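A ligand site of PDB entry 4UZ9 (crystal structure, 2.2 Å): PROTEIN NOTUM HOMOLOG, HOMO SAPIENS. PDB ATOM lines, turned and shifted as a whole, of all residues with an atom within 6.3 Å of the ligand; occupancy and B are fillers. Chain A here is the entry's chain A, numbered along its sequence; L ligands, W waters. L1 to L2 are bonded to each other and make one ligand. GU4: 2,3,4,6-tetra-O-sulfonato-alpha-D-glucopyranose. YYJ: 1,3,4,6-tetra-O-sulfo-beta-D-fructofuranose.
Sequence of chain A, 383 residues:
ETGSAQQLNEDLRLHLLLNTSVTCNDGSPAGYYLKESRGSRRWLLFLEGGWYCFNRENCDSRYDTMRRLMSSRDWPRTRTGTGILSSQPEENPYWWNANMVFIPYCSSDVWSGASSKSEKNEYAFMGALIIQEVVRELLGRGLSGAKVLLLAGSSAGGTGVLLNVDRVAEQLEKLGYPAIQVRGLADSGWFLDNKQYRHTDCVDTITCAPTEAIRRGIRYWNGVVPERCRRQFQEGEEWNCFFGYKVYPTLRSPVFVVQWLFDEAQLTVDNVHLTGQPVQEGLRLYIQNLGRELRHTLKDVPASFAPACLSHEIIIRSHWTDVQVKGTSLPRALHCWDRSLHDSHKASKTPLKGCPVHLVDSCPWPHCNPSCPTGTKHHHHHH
The side-chain amide nitrogen (ND2) of Asn 97 lies within hydrogen-bond range of an oxygen (O3S6) of YYJ L2, at 3.4 Å. A ring nitrogen (ND1) of His 342 lies within hydrogen-bond range of an oxygen (O10) of GU4 L1 (3.0 Å). NH1 of Arg 41 is in salt-bridge range of O25 of GU4 L1. An oxygen (O2S6) of YYJ L2 sits at hydrogen-bond distance from the side-chain hydroxyl (OG) of Ser 40. The side-chain amino group (NZ) of Lys 147 is in salt-bridge range of an oxygen (O29) of GU4 L1. NH2 of Arg 42 lies within salt-bridge range of O3S1 of YYJ L2 (3.0 Å).
Residues that only touch the ligand: His 335 (3.5 Å), Arg 339 (3.7 Å), Asp 338 (3.8 Å), Gln 181 (3.8 Å) and Val 148 (3.9 Å). Hydrophobic or aromatic side chains within 4 Å of the ligand: Val 148, His 335 and His 342.
The backbone carbonyl oxygen of Lys 147 lies within hydrogen-bond range of the backbone NH of Gln 181 (2.9 Å). OD1 of Asp 338 lies within salt-bridge range of NH1 of Arg 183 (3.8 Å). NE2 of His 335 is in hydrogen-bond range of NH1 of Arg 339. OG of Ser 40 is in hydrogen-bond range of N of Arg 42 (3.1 Å). The side-chain amide nitrogen (NE2) of Gln 181 sits close to the guanidinium group (NH2) of Arg 183. The backbone NH of Lys 147 lies within hydrogen-bond range of the backbone carbonyl oxygen of Arg 41, at 2.9 Å. The backbone NH (N) of Val 148 lies within hydrogen-bond range of the backbone carbonyl oxygen (O) of Arg 41 (3.3 Å).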
ATOM      1  N   GLY A  39      16.663  19.106  -7.549  1.00  0.00           N
ATOM      2  CA  GLY A  39      16.244  18.925  -6.157  1.00  0.00           C
ATOM      3  C   GLY A  39      17.325  18.402  -5.227  1.00  0.00           C
ATOM      4  O   GLY A  39      17.048  18.054  -4.075  1.00  0.00           O
ATOM      5  N   SER A  40      18.571  18.338  -5.675  1.00  0.00           N
ATOM      6  CA  SER A  40      19.635  17.768  -4.870  1.00  0.00           C
ATOM      7  C   SER A  40      20.825  18.676  -4.852  1.00  0.00           C
ATOM      8  O   SER A  40      21.121  19.276  -5.864  1.00  0.00           O
ATOM      9  CB  SER A  40      20.084  16.435  -5.470  1.00  0.00           C
ATOM     10  OG  SER A  40      21.157  15.924  -4.697  1.00  0.00           O
ATOM     11  N   ARG A  41      21.533  18.672  -3.732  1.00  0.00           N
ATOM     12  CA  ARG A  41      22.751  19.437  -3.563  1.00  0.00           C
ATOM     13  C   ARG A  41      24.017  18.541  -3.456  1.00  0.00           C
ATOM     14  O   ARG A  41      25.111  18.981  -3.102  1.00  0.00           O
ATOM     15  CB  ARG A  41      22.578  20.381  -2.374  1.00  0.00           C
ATOM     16  CG  ARG A  41      21.764  21.639  -2.784  1.00  0.00           C
ATOM     17  CD  ARG A  41      20.834  22.152  -1.705  1.00  0.00           C
ATOM     18  NE  ARG A  41      21.406  23.198  -0.879  1.00  0.00           N
ATOM     19  CZ  ARG A  41      21.431  23.236   0.472  1.00  0.00           C
ATOM     20  NH1 ARG A  41      20.936  22.256   1.241  1.00  0.00           N
ATOM     21  NH2 ARG A  41      21.972  24.305   1.064  1.00  0.00           N
ATOM     22  N   ARG A  42      23.845  17.278  -3.842  1.00  0.00           N
ATOM     23  CA  ARG A  42      24.910  16.296  -3.887  1.00  0.00           C
ATOM     24  C   ARG A  42      25.328  16.139  -5.325  1.00  0.00           C
ATOM     25  O   ARG A  42      24.507  16.070  -6.207  1.00  0.00           O
ATOM     26  CB  ARG A  42      24.406  14.964  -3.379  1.00  0.00           C
ATOM     27  CG  ARG A  42      23.724  15.024  -2.025  1.00  0.00           C
ATOM     28  CD  ARG A  42      24.554  14.354  -0.951  1.00  0.00           C
ATOM     29  NE  ARG A  42      23.763  13.967   0.205  1.00  0.00           N
ATOM     30  CZ  ARG A  42      23.326  12.725   0.460  1.00  0.00           C
ATOM     31  NH1 ARG A  42      23.603  11.720  -0.388  1.00  0.00           N
ATOM     32  NH2 ARG A  42      22.605  12.502   1.562  1.00  0.00           N
ATOM     33  N   TYR A  94      21.402   4.896  -1.782  1.00  0.00           N
ATOM     34  CA  TYR A  94      21.568   6.239  -1.126  1.00  0.00           C
ATOM     35  C   TYR A  94      21.900   7.447  -2.003  1.00  0.00           C
ATOM     36  O   TYR A  94      21.778   8.582  -1.551  1.00  0.00           O
ATOM     37  CB  TYR A  94      22.520   6.150   0.094  1.00  0.00           C
ATOM     38  CG  TYR A  94      22.080   5.052   1.017  1.00  0.00           C
ATOM     39  CD1 TYR A  94      22.499   3.742   0.801  1.00  0.00           C
ATOM     40  CD2 TYR A  94      21.180   5.289   2.054  1.00  0.00           C
ATOM     41  CE1 TYR A  94      22.057   2.696   1.598  1.00  0.00           C
ATOM     42  CE2 TYR A  94      20.724   4.248   2.870  1.00  0.00           C
ATOM     43  CZ  TYR A  94      21.178   2.944   2.626  1.00  0.00           C
ATOM     44  OH  TYR A  94      20.796   1.853   3.400  1.00  0.00           O
ATOM     45  N   TRP A  96      20.779   7.866  -5.402  1.00  0.00           N
ATOM     46  CA  TRP A  96      19.990   7.866  -6.637  1.00  0.00           C
ATOM     47  C   TRP A  96      19.547   9.266  -7.081  1.00  0.00           C
ATOM     48  O   TRP A  96      19.402   9.522  -8.279  1.00  0.00           O
ATOM     49  CB  TRP A  96      18.738   6.954  -6.489  1.00  0.00           C
ATOM     50  CG  TRP A  96      17.662   7.515  -5.547  1.00  0.00           C
ATOM     51  CD1 TRP A  96      17.531   7.280  -4.195  1.00  0.00           C
ATOM     52  CD2 TRP A  96      16.602   8.403  -5.898  1.00  0.00           C
ATOM     53  NE1 TRP A  96      16.459   7.984  -3.695  1.00  0.00           N
ATOM     54  CE2 TRP A  96      15.861   8.671  -4.716  1.00  0.00           C
ATOM     55  CE3 TRP A  96      16.186   8.994  -7.098  1.00  0.00           C
ATOM     56  CZ2 TRP A  96      14.752   9.500  -4.703  1.00  0.00           C
ATOM     57  CZ3 TRP A  96      15.070   9.839  -7.084  1.00  0.00           C
ATOM     58  CH2 TRP A  96      14.368  10.075  -5.897  1.00  0.00           C
ATOM     59  N   ASN A  97      19.331  10.180  -6.137  1.00  0.00           N
ATOM     60  CA  ASN A  97      18.765  11.465  -6.516  1.00  0.00           C
ATOM     61  C   ASN A  97      19.831  12.556  -6.729  1.00  0.00           C
ATOM     62  O   ASN A  97      19.482  13.743  -6.922  1.00  0.00           O
ATOM     63  CB  ASN A  97      17.804  11.949  -5.453  1.00  0.00           C
ATOM     64  CG  ASN A  97      16.837  13.001  -5.979  1.00  0.00           C
ATOM     65  OD1 ASN A  97      16.373  12.941  -7.137  1.00  0.00           O
ATOM     66  ND2 ASN A  97      16.565  13.983  -5.138  1.00  0.00           N
ATOM     67  N   ALA A  98      21.099  12.150  -6.702  1.00  0.00           N
ATOM     68  CA  ALA A  98      22.200  13.094  -6.870  1.00  0.00           C
ATOM     69  C   ALA A  98      22.370  13.564  -8.303  1.00  0.00           C
ATOM     70  O   ALA A  98      21.870  12.961  -9.235  1.00  0.00           O
ATOM     71  CB  ALA A  98      23.495  12.485  -6.350  1.00  0.00           C
ATOM     72  N   LYS A 147      26.451  21.166  -1.833  1.00  0.00           N
ATOM     73  CA  LYS A 147      26.942  20.985  -0.457  1.00  0.00           C
ATOM     74  C   LYS A 147      27.937  19.813  -0.340  1.00  0.00           C
ATOM     75  O   LYS A 147      28.783  19.771   0.540  1.00  0.00           O
ATOM     76  CB  LYS A 147      25.753  20.718   0.505  1.00  0.00           C
ATOM     77  CG  LYS A 147      25.115  21.946   1.192  1.00  0.00           C
ATOM     78  CD  LYS A 147      25.007  21.772   2.716  1.00  0.00           C
ATOM     79  CE  LYS A 147      23.855  22.544   3.363  1.00  0.00           C
ATOM     80  NZ  LYS A 147      24.123  23.968   3.777  1.00  0.00           N
ATOM     81  N   VAL A 148      27.831  18.829  -1.230  1.00  0.00           N
ATOM     82  CA  VAL A 148      28.815  17.714  -1.298  1.00  0.00           C
ATOM     83  C   VAL A 148      29.182  17.424  -2.738  1.00  0.00           C
ATOM     84  O   VAL A 148      28.295  17.380  -3.638  1.00  0.00           O
ATOM     85  CB  VAL A 148      28.231  16.426  -0.700  1.00  0.00           C
ATOM     86  CG1 VAL A 148      29.235  15.273  -0.725  1.00  0.00           C
ATOM     87  CG2 VAL A 148      27.809  16.694   0.710  1.00  0.00           C
ATOM     88  N   GLN A 181      31.597  20.439   0.431  1.00  0.00           N
ATOM     89  CA  GLN A 181      32.414  19.407   1.044  1.00  0.00           C
ATOM     90  C   GLN A 181      32.906  18.398  -0.020  1.00  0.00           C
ATOM     91  O   GLN A 181      32.093  17.634  -0.573  1.00  0.00           O
ATOM     92  CB  GLN A 181      31.616  18.706   2.123  1.00  0.00           C
ATOM     93  CG  GLN A 181      31.046  19.620   3.220  1.00  0.00           C
ATOM     94  CD  GLN A 181      30.280  18.795   4.259  1.00  0.00           C
ATOM     95  OE1 GLN A 181      29.065  18.899   4.397  1.00  0.00           O
ATOM     96  NE2 GLN A 181      31.008  17.920   4.950  1.00  0.00           N
ATOM     97  N   ARG A 183      34.923  15.115  -1.069  1.00  0.00           N
ATOM     98  CA  ARG A 183      35.219  13.784  -0.552  1.00  0.00           C
ATOM     99  C   ARG A 183      35.628  12.840  -1.703  1.00  0.00           C
ATOM    100  O   ARG A 183      35.248  13.048  -2.850  1.00  0.00           O
ATOM    101  CB  ARG A 183      33.979  13.185   0.109  1.00  0.00           C
ATOM    102  CG  ARG A 183      33.370  14.052   1.203  1.00  0.00           C
ATOM    103  CD  ARG A 183      31.965  13.526   1.557  1.00  0.00           C
ATOM    104  NE  ARG A 183      31.320  14.323   2.605  1.00  0.00           N
ATOM    105  CZ  ARG A 183      30.051  14.217   2.963  1.00  0.00           C
ATOM    106  NH1 ARG A 183      29.265  13.322   2.418  1.00  0.00           N
ATOM    107  NH2 ARG A 183      29.562  15.005   3.905  1.00  0.00           N
ATOM    108  N   HIS A 335      26.856   4.889   3.171  1.00  0.00           N
ATOM    109  CA  HIS A 335      25.892   5.696   3.921  1.00  0.00           C
ATOM    110  C   HIS A 335      26.395   5.964   5.363  1.00  0.00           C
ATOM    111  O   HIS A 335      26.183   7.074   5.880  1.00  0.00           O
ATOM    112  CB  HIS A 335      24.476   5.056   3.970  1.00  0.00           C
ATOM    113  CG  HIS A 335      23.533   5.725   4.942  1.00  0.00           C
ATOM    114  ND1 HIS A 335      22.926   6.948   4.691  1.00  0.00           N
ATOM    115  CD2 HIS A 335      23.110   5.347   6.180  1.00  0.00           C
ATOM    116  CE1 HIS A 335      22.190   7.291   5.725  1.00  0.00           C
ATOM    117  NE2 HIS A 335      22.281   6.340   6.648  1.00  0.00           N
ATOM    118  N   ASP A 338      29.177   8.653   5.143  1.00  0.00           N
ATOM    119  CA  ASP A 338      28.524   9.954   5.041  1.00  0.00           C
ATOM    120  C   ASP A 338      27.975  10.441   6.353  1.00  0.00           C
ATOM    121  O   ASP A 338      28.183  11.601   6.702  1.00  0.00           O
ATOM    122  CB  ASP A 338      27.350   9.911   4.075  1.00  0.00           C
ATOM    123  CG  ASP A 338      27.769   9.655   2.650  1.00  0.00           C
ATOM    124  OD1 ASP A 338      28.991   9.581   2.393  1.00  0.00           O
ATOM    125  OD2 ASP A 338      26.864   9.534   1.797  1.00  0.00           O
ATOM    126  N   ARG A 339      27.251   9.590   7.079  1.00  0.00           N
ATOM    127  CA  ARG A 339      26.668   9.961   8.373  1.00  0.00           C
ATOM    128  C   ARG A 339      27.772  10.420   9.331  1.00  0.00           C
ATOM    129  O   ARG A 339      27.653  11.453   9.999  1.00  0.00           O
ATOM    130  CB  ARG A 339      25.876   8.797   8.997  1.00  0.00           C
ATOM    131  CG  ARG A 339      25.081   9.183  10.257  1.00  0.00           C
ATOM    132  CD  ARG A 339      23.676   8.580  10.320  1.00  0.00           C
ATOM    133  NE  ARG A 339      23.595   7.367  11.125  1.00  0.00           N
ATOM    134  CZ  ARG A 339      23.409   6.154  10.640  1.00  0.00           C
ATOM    135  NH1 ARG A 339      23.295   5.988   9.336  1.00  0.00           N
ATOM    136  NH2 ARG A 339      23.335   5.107  11.459  1.00  0.00           N
ATOM    137  N   SER A 340      28.862   9.656   9.362  1.00  0.00           N
ATOM    138  CA  SER A 340      30.020  10.000  10.181  1.00  0.00           C
ATOM    139  C   SER A 340      30.657  11.331   9.785  1.00  0.00           C
ATOM    140  O   SER A 340      31.273  11.969  10.603  1.00  0.00           O
ATOM    141  CB  SER A 340      31.079   8.885  10.109  1.00  0.00           C
ATOM    142  OG  SER A 340      31.881   9.049   8.956  1.00  0.00           O
ATOM    143  N   LEU A 341      30.542  11.750   8.540  1.00  0.00           N
ATOM    144  CA  LEU A 341      31.097  13.051   8.138  1.00  0.00           C
ATOM    145  C   LEU A 341      30.153  14.212   8.375  1.00  0.00           C
ATOM    146  O   LEU A 341      30.589  15.334   8.400  1.00  0.00           O
ATOM    147  CB  LEU A 341      31.517  13.040   6.673  1.00  0.00           C
ATOM    148  CG  LEU A 341      32.629  12.048   6.326  1.00  0.00           C
ATOM    149  CD1 LEU A 341      32.873  12.076   4.826  1.00  0.00           C
ATOM    150  CD2 LEU A 341      33.921  12.348   7.082  1.00  0.00           C
ATOM    151  N   HIS A 342      28.873  13.927   8.518  1.00  0.00           N
ATOM    152  CA  HIS A 342      27.858  14.958   8.759  1.00  0.00           C
ATOM    153  C   HIS A 342      28.011  15.598  10.168  1.00  0.00           C
ATOM    154  O   HIS A 342      27.586  16.736  10.378  1.00  0.00           O
ATOM    155  CB  HIS A 342      26.458  14.354   8.549  1.00  0.00           C
ATOM    156  CG  HIS A 342      25.359  15.370   8.474  1.00  0.00           C
ATOM    157  ND1 HIS A 342      25.129  16.135   7.344  1.00  0.00           N
ATOM    158  CD2 HIS A 342      24.411  15.732   9.375  1.00  0.00           C
ATOM    159  CE1 HIS A 342      24.095  16.933   7.562  1.00  0.00           C
ATOM    160  NE2 HIS A 342      23.648  16.713   8.787  1.00  0.00           N
HETATM  161  C1  GU4 L   1      21.393  16.790   3.225  1.00  0.00           C
HETATM  162  O5  GU4 L   1      20.352  17.339   2.436  1.00  0.00           O
HETATM  163  C5  GU4 L   1      19.429  18.073   3.250  1.00  0.00           C
HETATM  164  C6  GU4 L   1      18.283  18.590   2.381  1.00  0.00           C
HETATM  165  O6  GU4 L   1      17.620  17.456   1.803  1.00  0.00           O
HETATM  166  S6  GU4 L   1      16.210  16.958   2.193  1.00  0.00           S
HETATM  167  O22 GU4 L   1      15.727  16.040   1.191  1.00  0.00           O
HETATM  168  O23 GU4 L   1      15.239  18.284   2.244  1.00  0.00           O
HETATM  169  O21 GU4 L   1      16.221  16.240   3.445  1.00  0.00           O
HETATM  170  C4  GU4 L   1      20.161  19.190   3.980  1.00  0.00           C
HETATM  171  O4  GU4 L   1      19.300  19.671   4.994  1.00  0.00           O
HETATM  172  S4  GU4 L   1      19.038  21.168   5.025  1.00  0.00           S
HETATM  173  O25 GU4 L   1      20.251  21.896   4.741  1.00  0.00           O
HETATM  174  O26 GU4 L   1      17.871  21.503   3.916  1.00  0.00           O
HETATM  175  O24 GU4 L   1      18.604  21.494   6.340  1.00  0.00           O
HETATM  176  C3  GU4 L   1      21.486  18.806   4.656  1.00  0.00           C
HETATM  177  O3  GU4 L   1      22.257  19.983   4.897  1.00  0.00           O
HETATM  178  S3  GU4 L   1      22.891  20.326   6.253  1.00  0.00           S
HETATM  179  O28 GU4 L   1      22.300  19.560   7.314  1.00  0.00           O
HETATM  180  O29 GU4 L   1      22.619  21.724   6.428  1.00  0.00           O
HETATM  181  O27 GU4 L   1      24.504  20.047   6.241  1.00  0.00           O
HETATM  182  C2  GU4 L   1      22.298  17.900   3.745  1.00  0.00           C
HETATM  183  O2  GU4 L   1      23.457  17.380   4.428  1.00  0.00           O
HETATM  184  S2  GU4 L   1      24.746  17.143   3.603  1.00  0.00           S
HETATM  185  O11 GU4 L   1      24.454  16.220   2.543  1.00  0.00           O
HETATM  186  O12 GU4 L   1      25.131  18.402   3.025  1.00  0.00           O
HETATM  187  O10 GU4 L   1      25.957  16.656   4.558  1.00  0.00           O
HETATM  188  C1  YYJ L   2      22.410  14.379   4.892  1.00  0.00           C
HETATM  189  C2  YYJ L   2      21.035  14.694   4.288  1.00  0.00           C
HETATM  190  C3  YYJ L   2      19.835  14.111   5.031  1.00  0.00           C
HETATM  191  C4  YYJ L   2      18.845  13.809   3.899  1.00  0.00           C
HETATM  192  C5  YYJ L   2      19.691  13.609   2.620  1.00  0.00           C
HETATM  193  C6  YYJ L   2      19.085  14.195   1.328  1.00  0.00           C
HETATM  194  O1  YYJ L   2      22.426  13.083   5.509  1.00  0.00           O
HETATM  195 O1S1 YYJ L   2      24.388  12.083   6.391  1.00  0.00           O
HETATM  196 O1S3 YYJ L   2      19.053  14.358   8.357  1.00  0.00           O
HETATM  197 O1S4 YYJ L   2      16.790  10.601   3.813  1.00  0.00           O
HETATM  198 O1S6 YYJ L   2      19.446  15.787  -1.021  1.00  0.00           O
HETATM  199  O2  YYJ L   2      20.842  16.095   4.345  1.00  0.00           O
HETATM  200 O2S1 YYJ L   2      22.876  10.710   5.241  1.00  0.00           O
HETATM  201 O2S3 YYJ L   2      20.036  16.468   7.995  1.00  0.00           O
HETATM  202 O2S4 YYJ L   2      15.798  12.688   3.304  1.00  0.00           O
HETATM  203 O2S6 YYJ L   2      20.386  14.086  -2.324  1.00  0.00           O
HETATM  204  O3  YYJ L   2      19.422  15.034   6.050  1.00  0.00           O
HETATM  205 O3S1 YYJ L   2      24.364  12.303   3.926  1.00  0.00           O
HETATM  206 O3S3 YYJ L   2      21.430  14.520   7.855  1.00  0.00           O
HETATM  207 O3S4 YYJ L   2      17.613  11.675   1.771  1.00  0.00           O
HETATM  208 O3S6 YYJ L   2      17.945  14.017  -1.994  1.00  0.00           O
HETATM  209  O4  YYJ L   2      18.095  12.619   4.211  1.00  0.00           O
HETATM  210  O5  YYJ L   2      20.954  14.227   2.922  1.00  0.00           O
HETATM  211  O6  YYJ L   2      19.618  13.636   0.092  1.00  0.00           O
HETATM  212  S1  YYJ L   2      23.501  12.011   5.276  1.00  0.00           S
HETATM  213  S3  YYJ L   2      19.952  15.112   7.530  1.00  0.00           S
HETATM  214  S4  YYJ L   2      17.035  11.919   3.298  1.00  0.00           S
HETATM  215  S6  YYJ L   2      19.389  14.348  -1.272  1.00  0.00           S
HETATM  216  O   HOH W   1      16.381  13.539   7.931  1.00  0.00           O
HETATM  217  O   HOH W   2      15.910  14.327   5.570  1.00  0.00           O
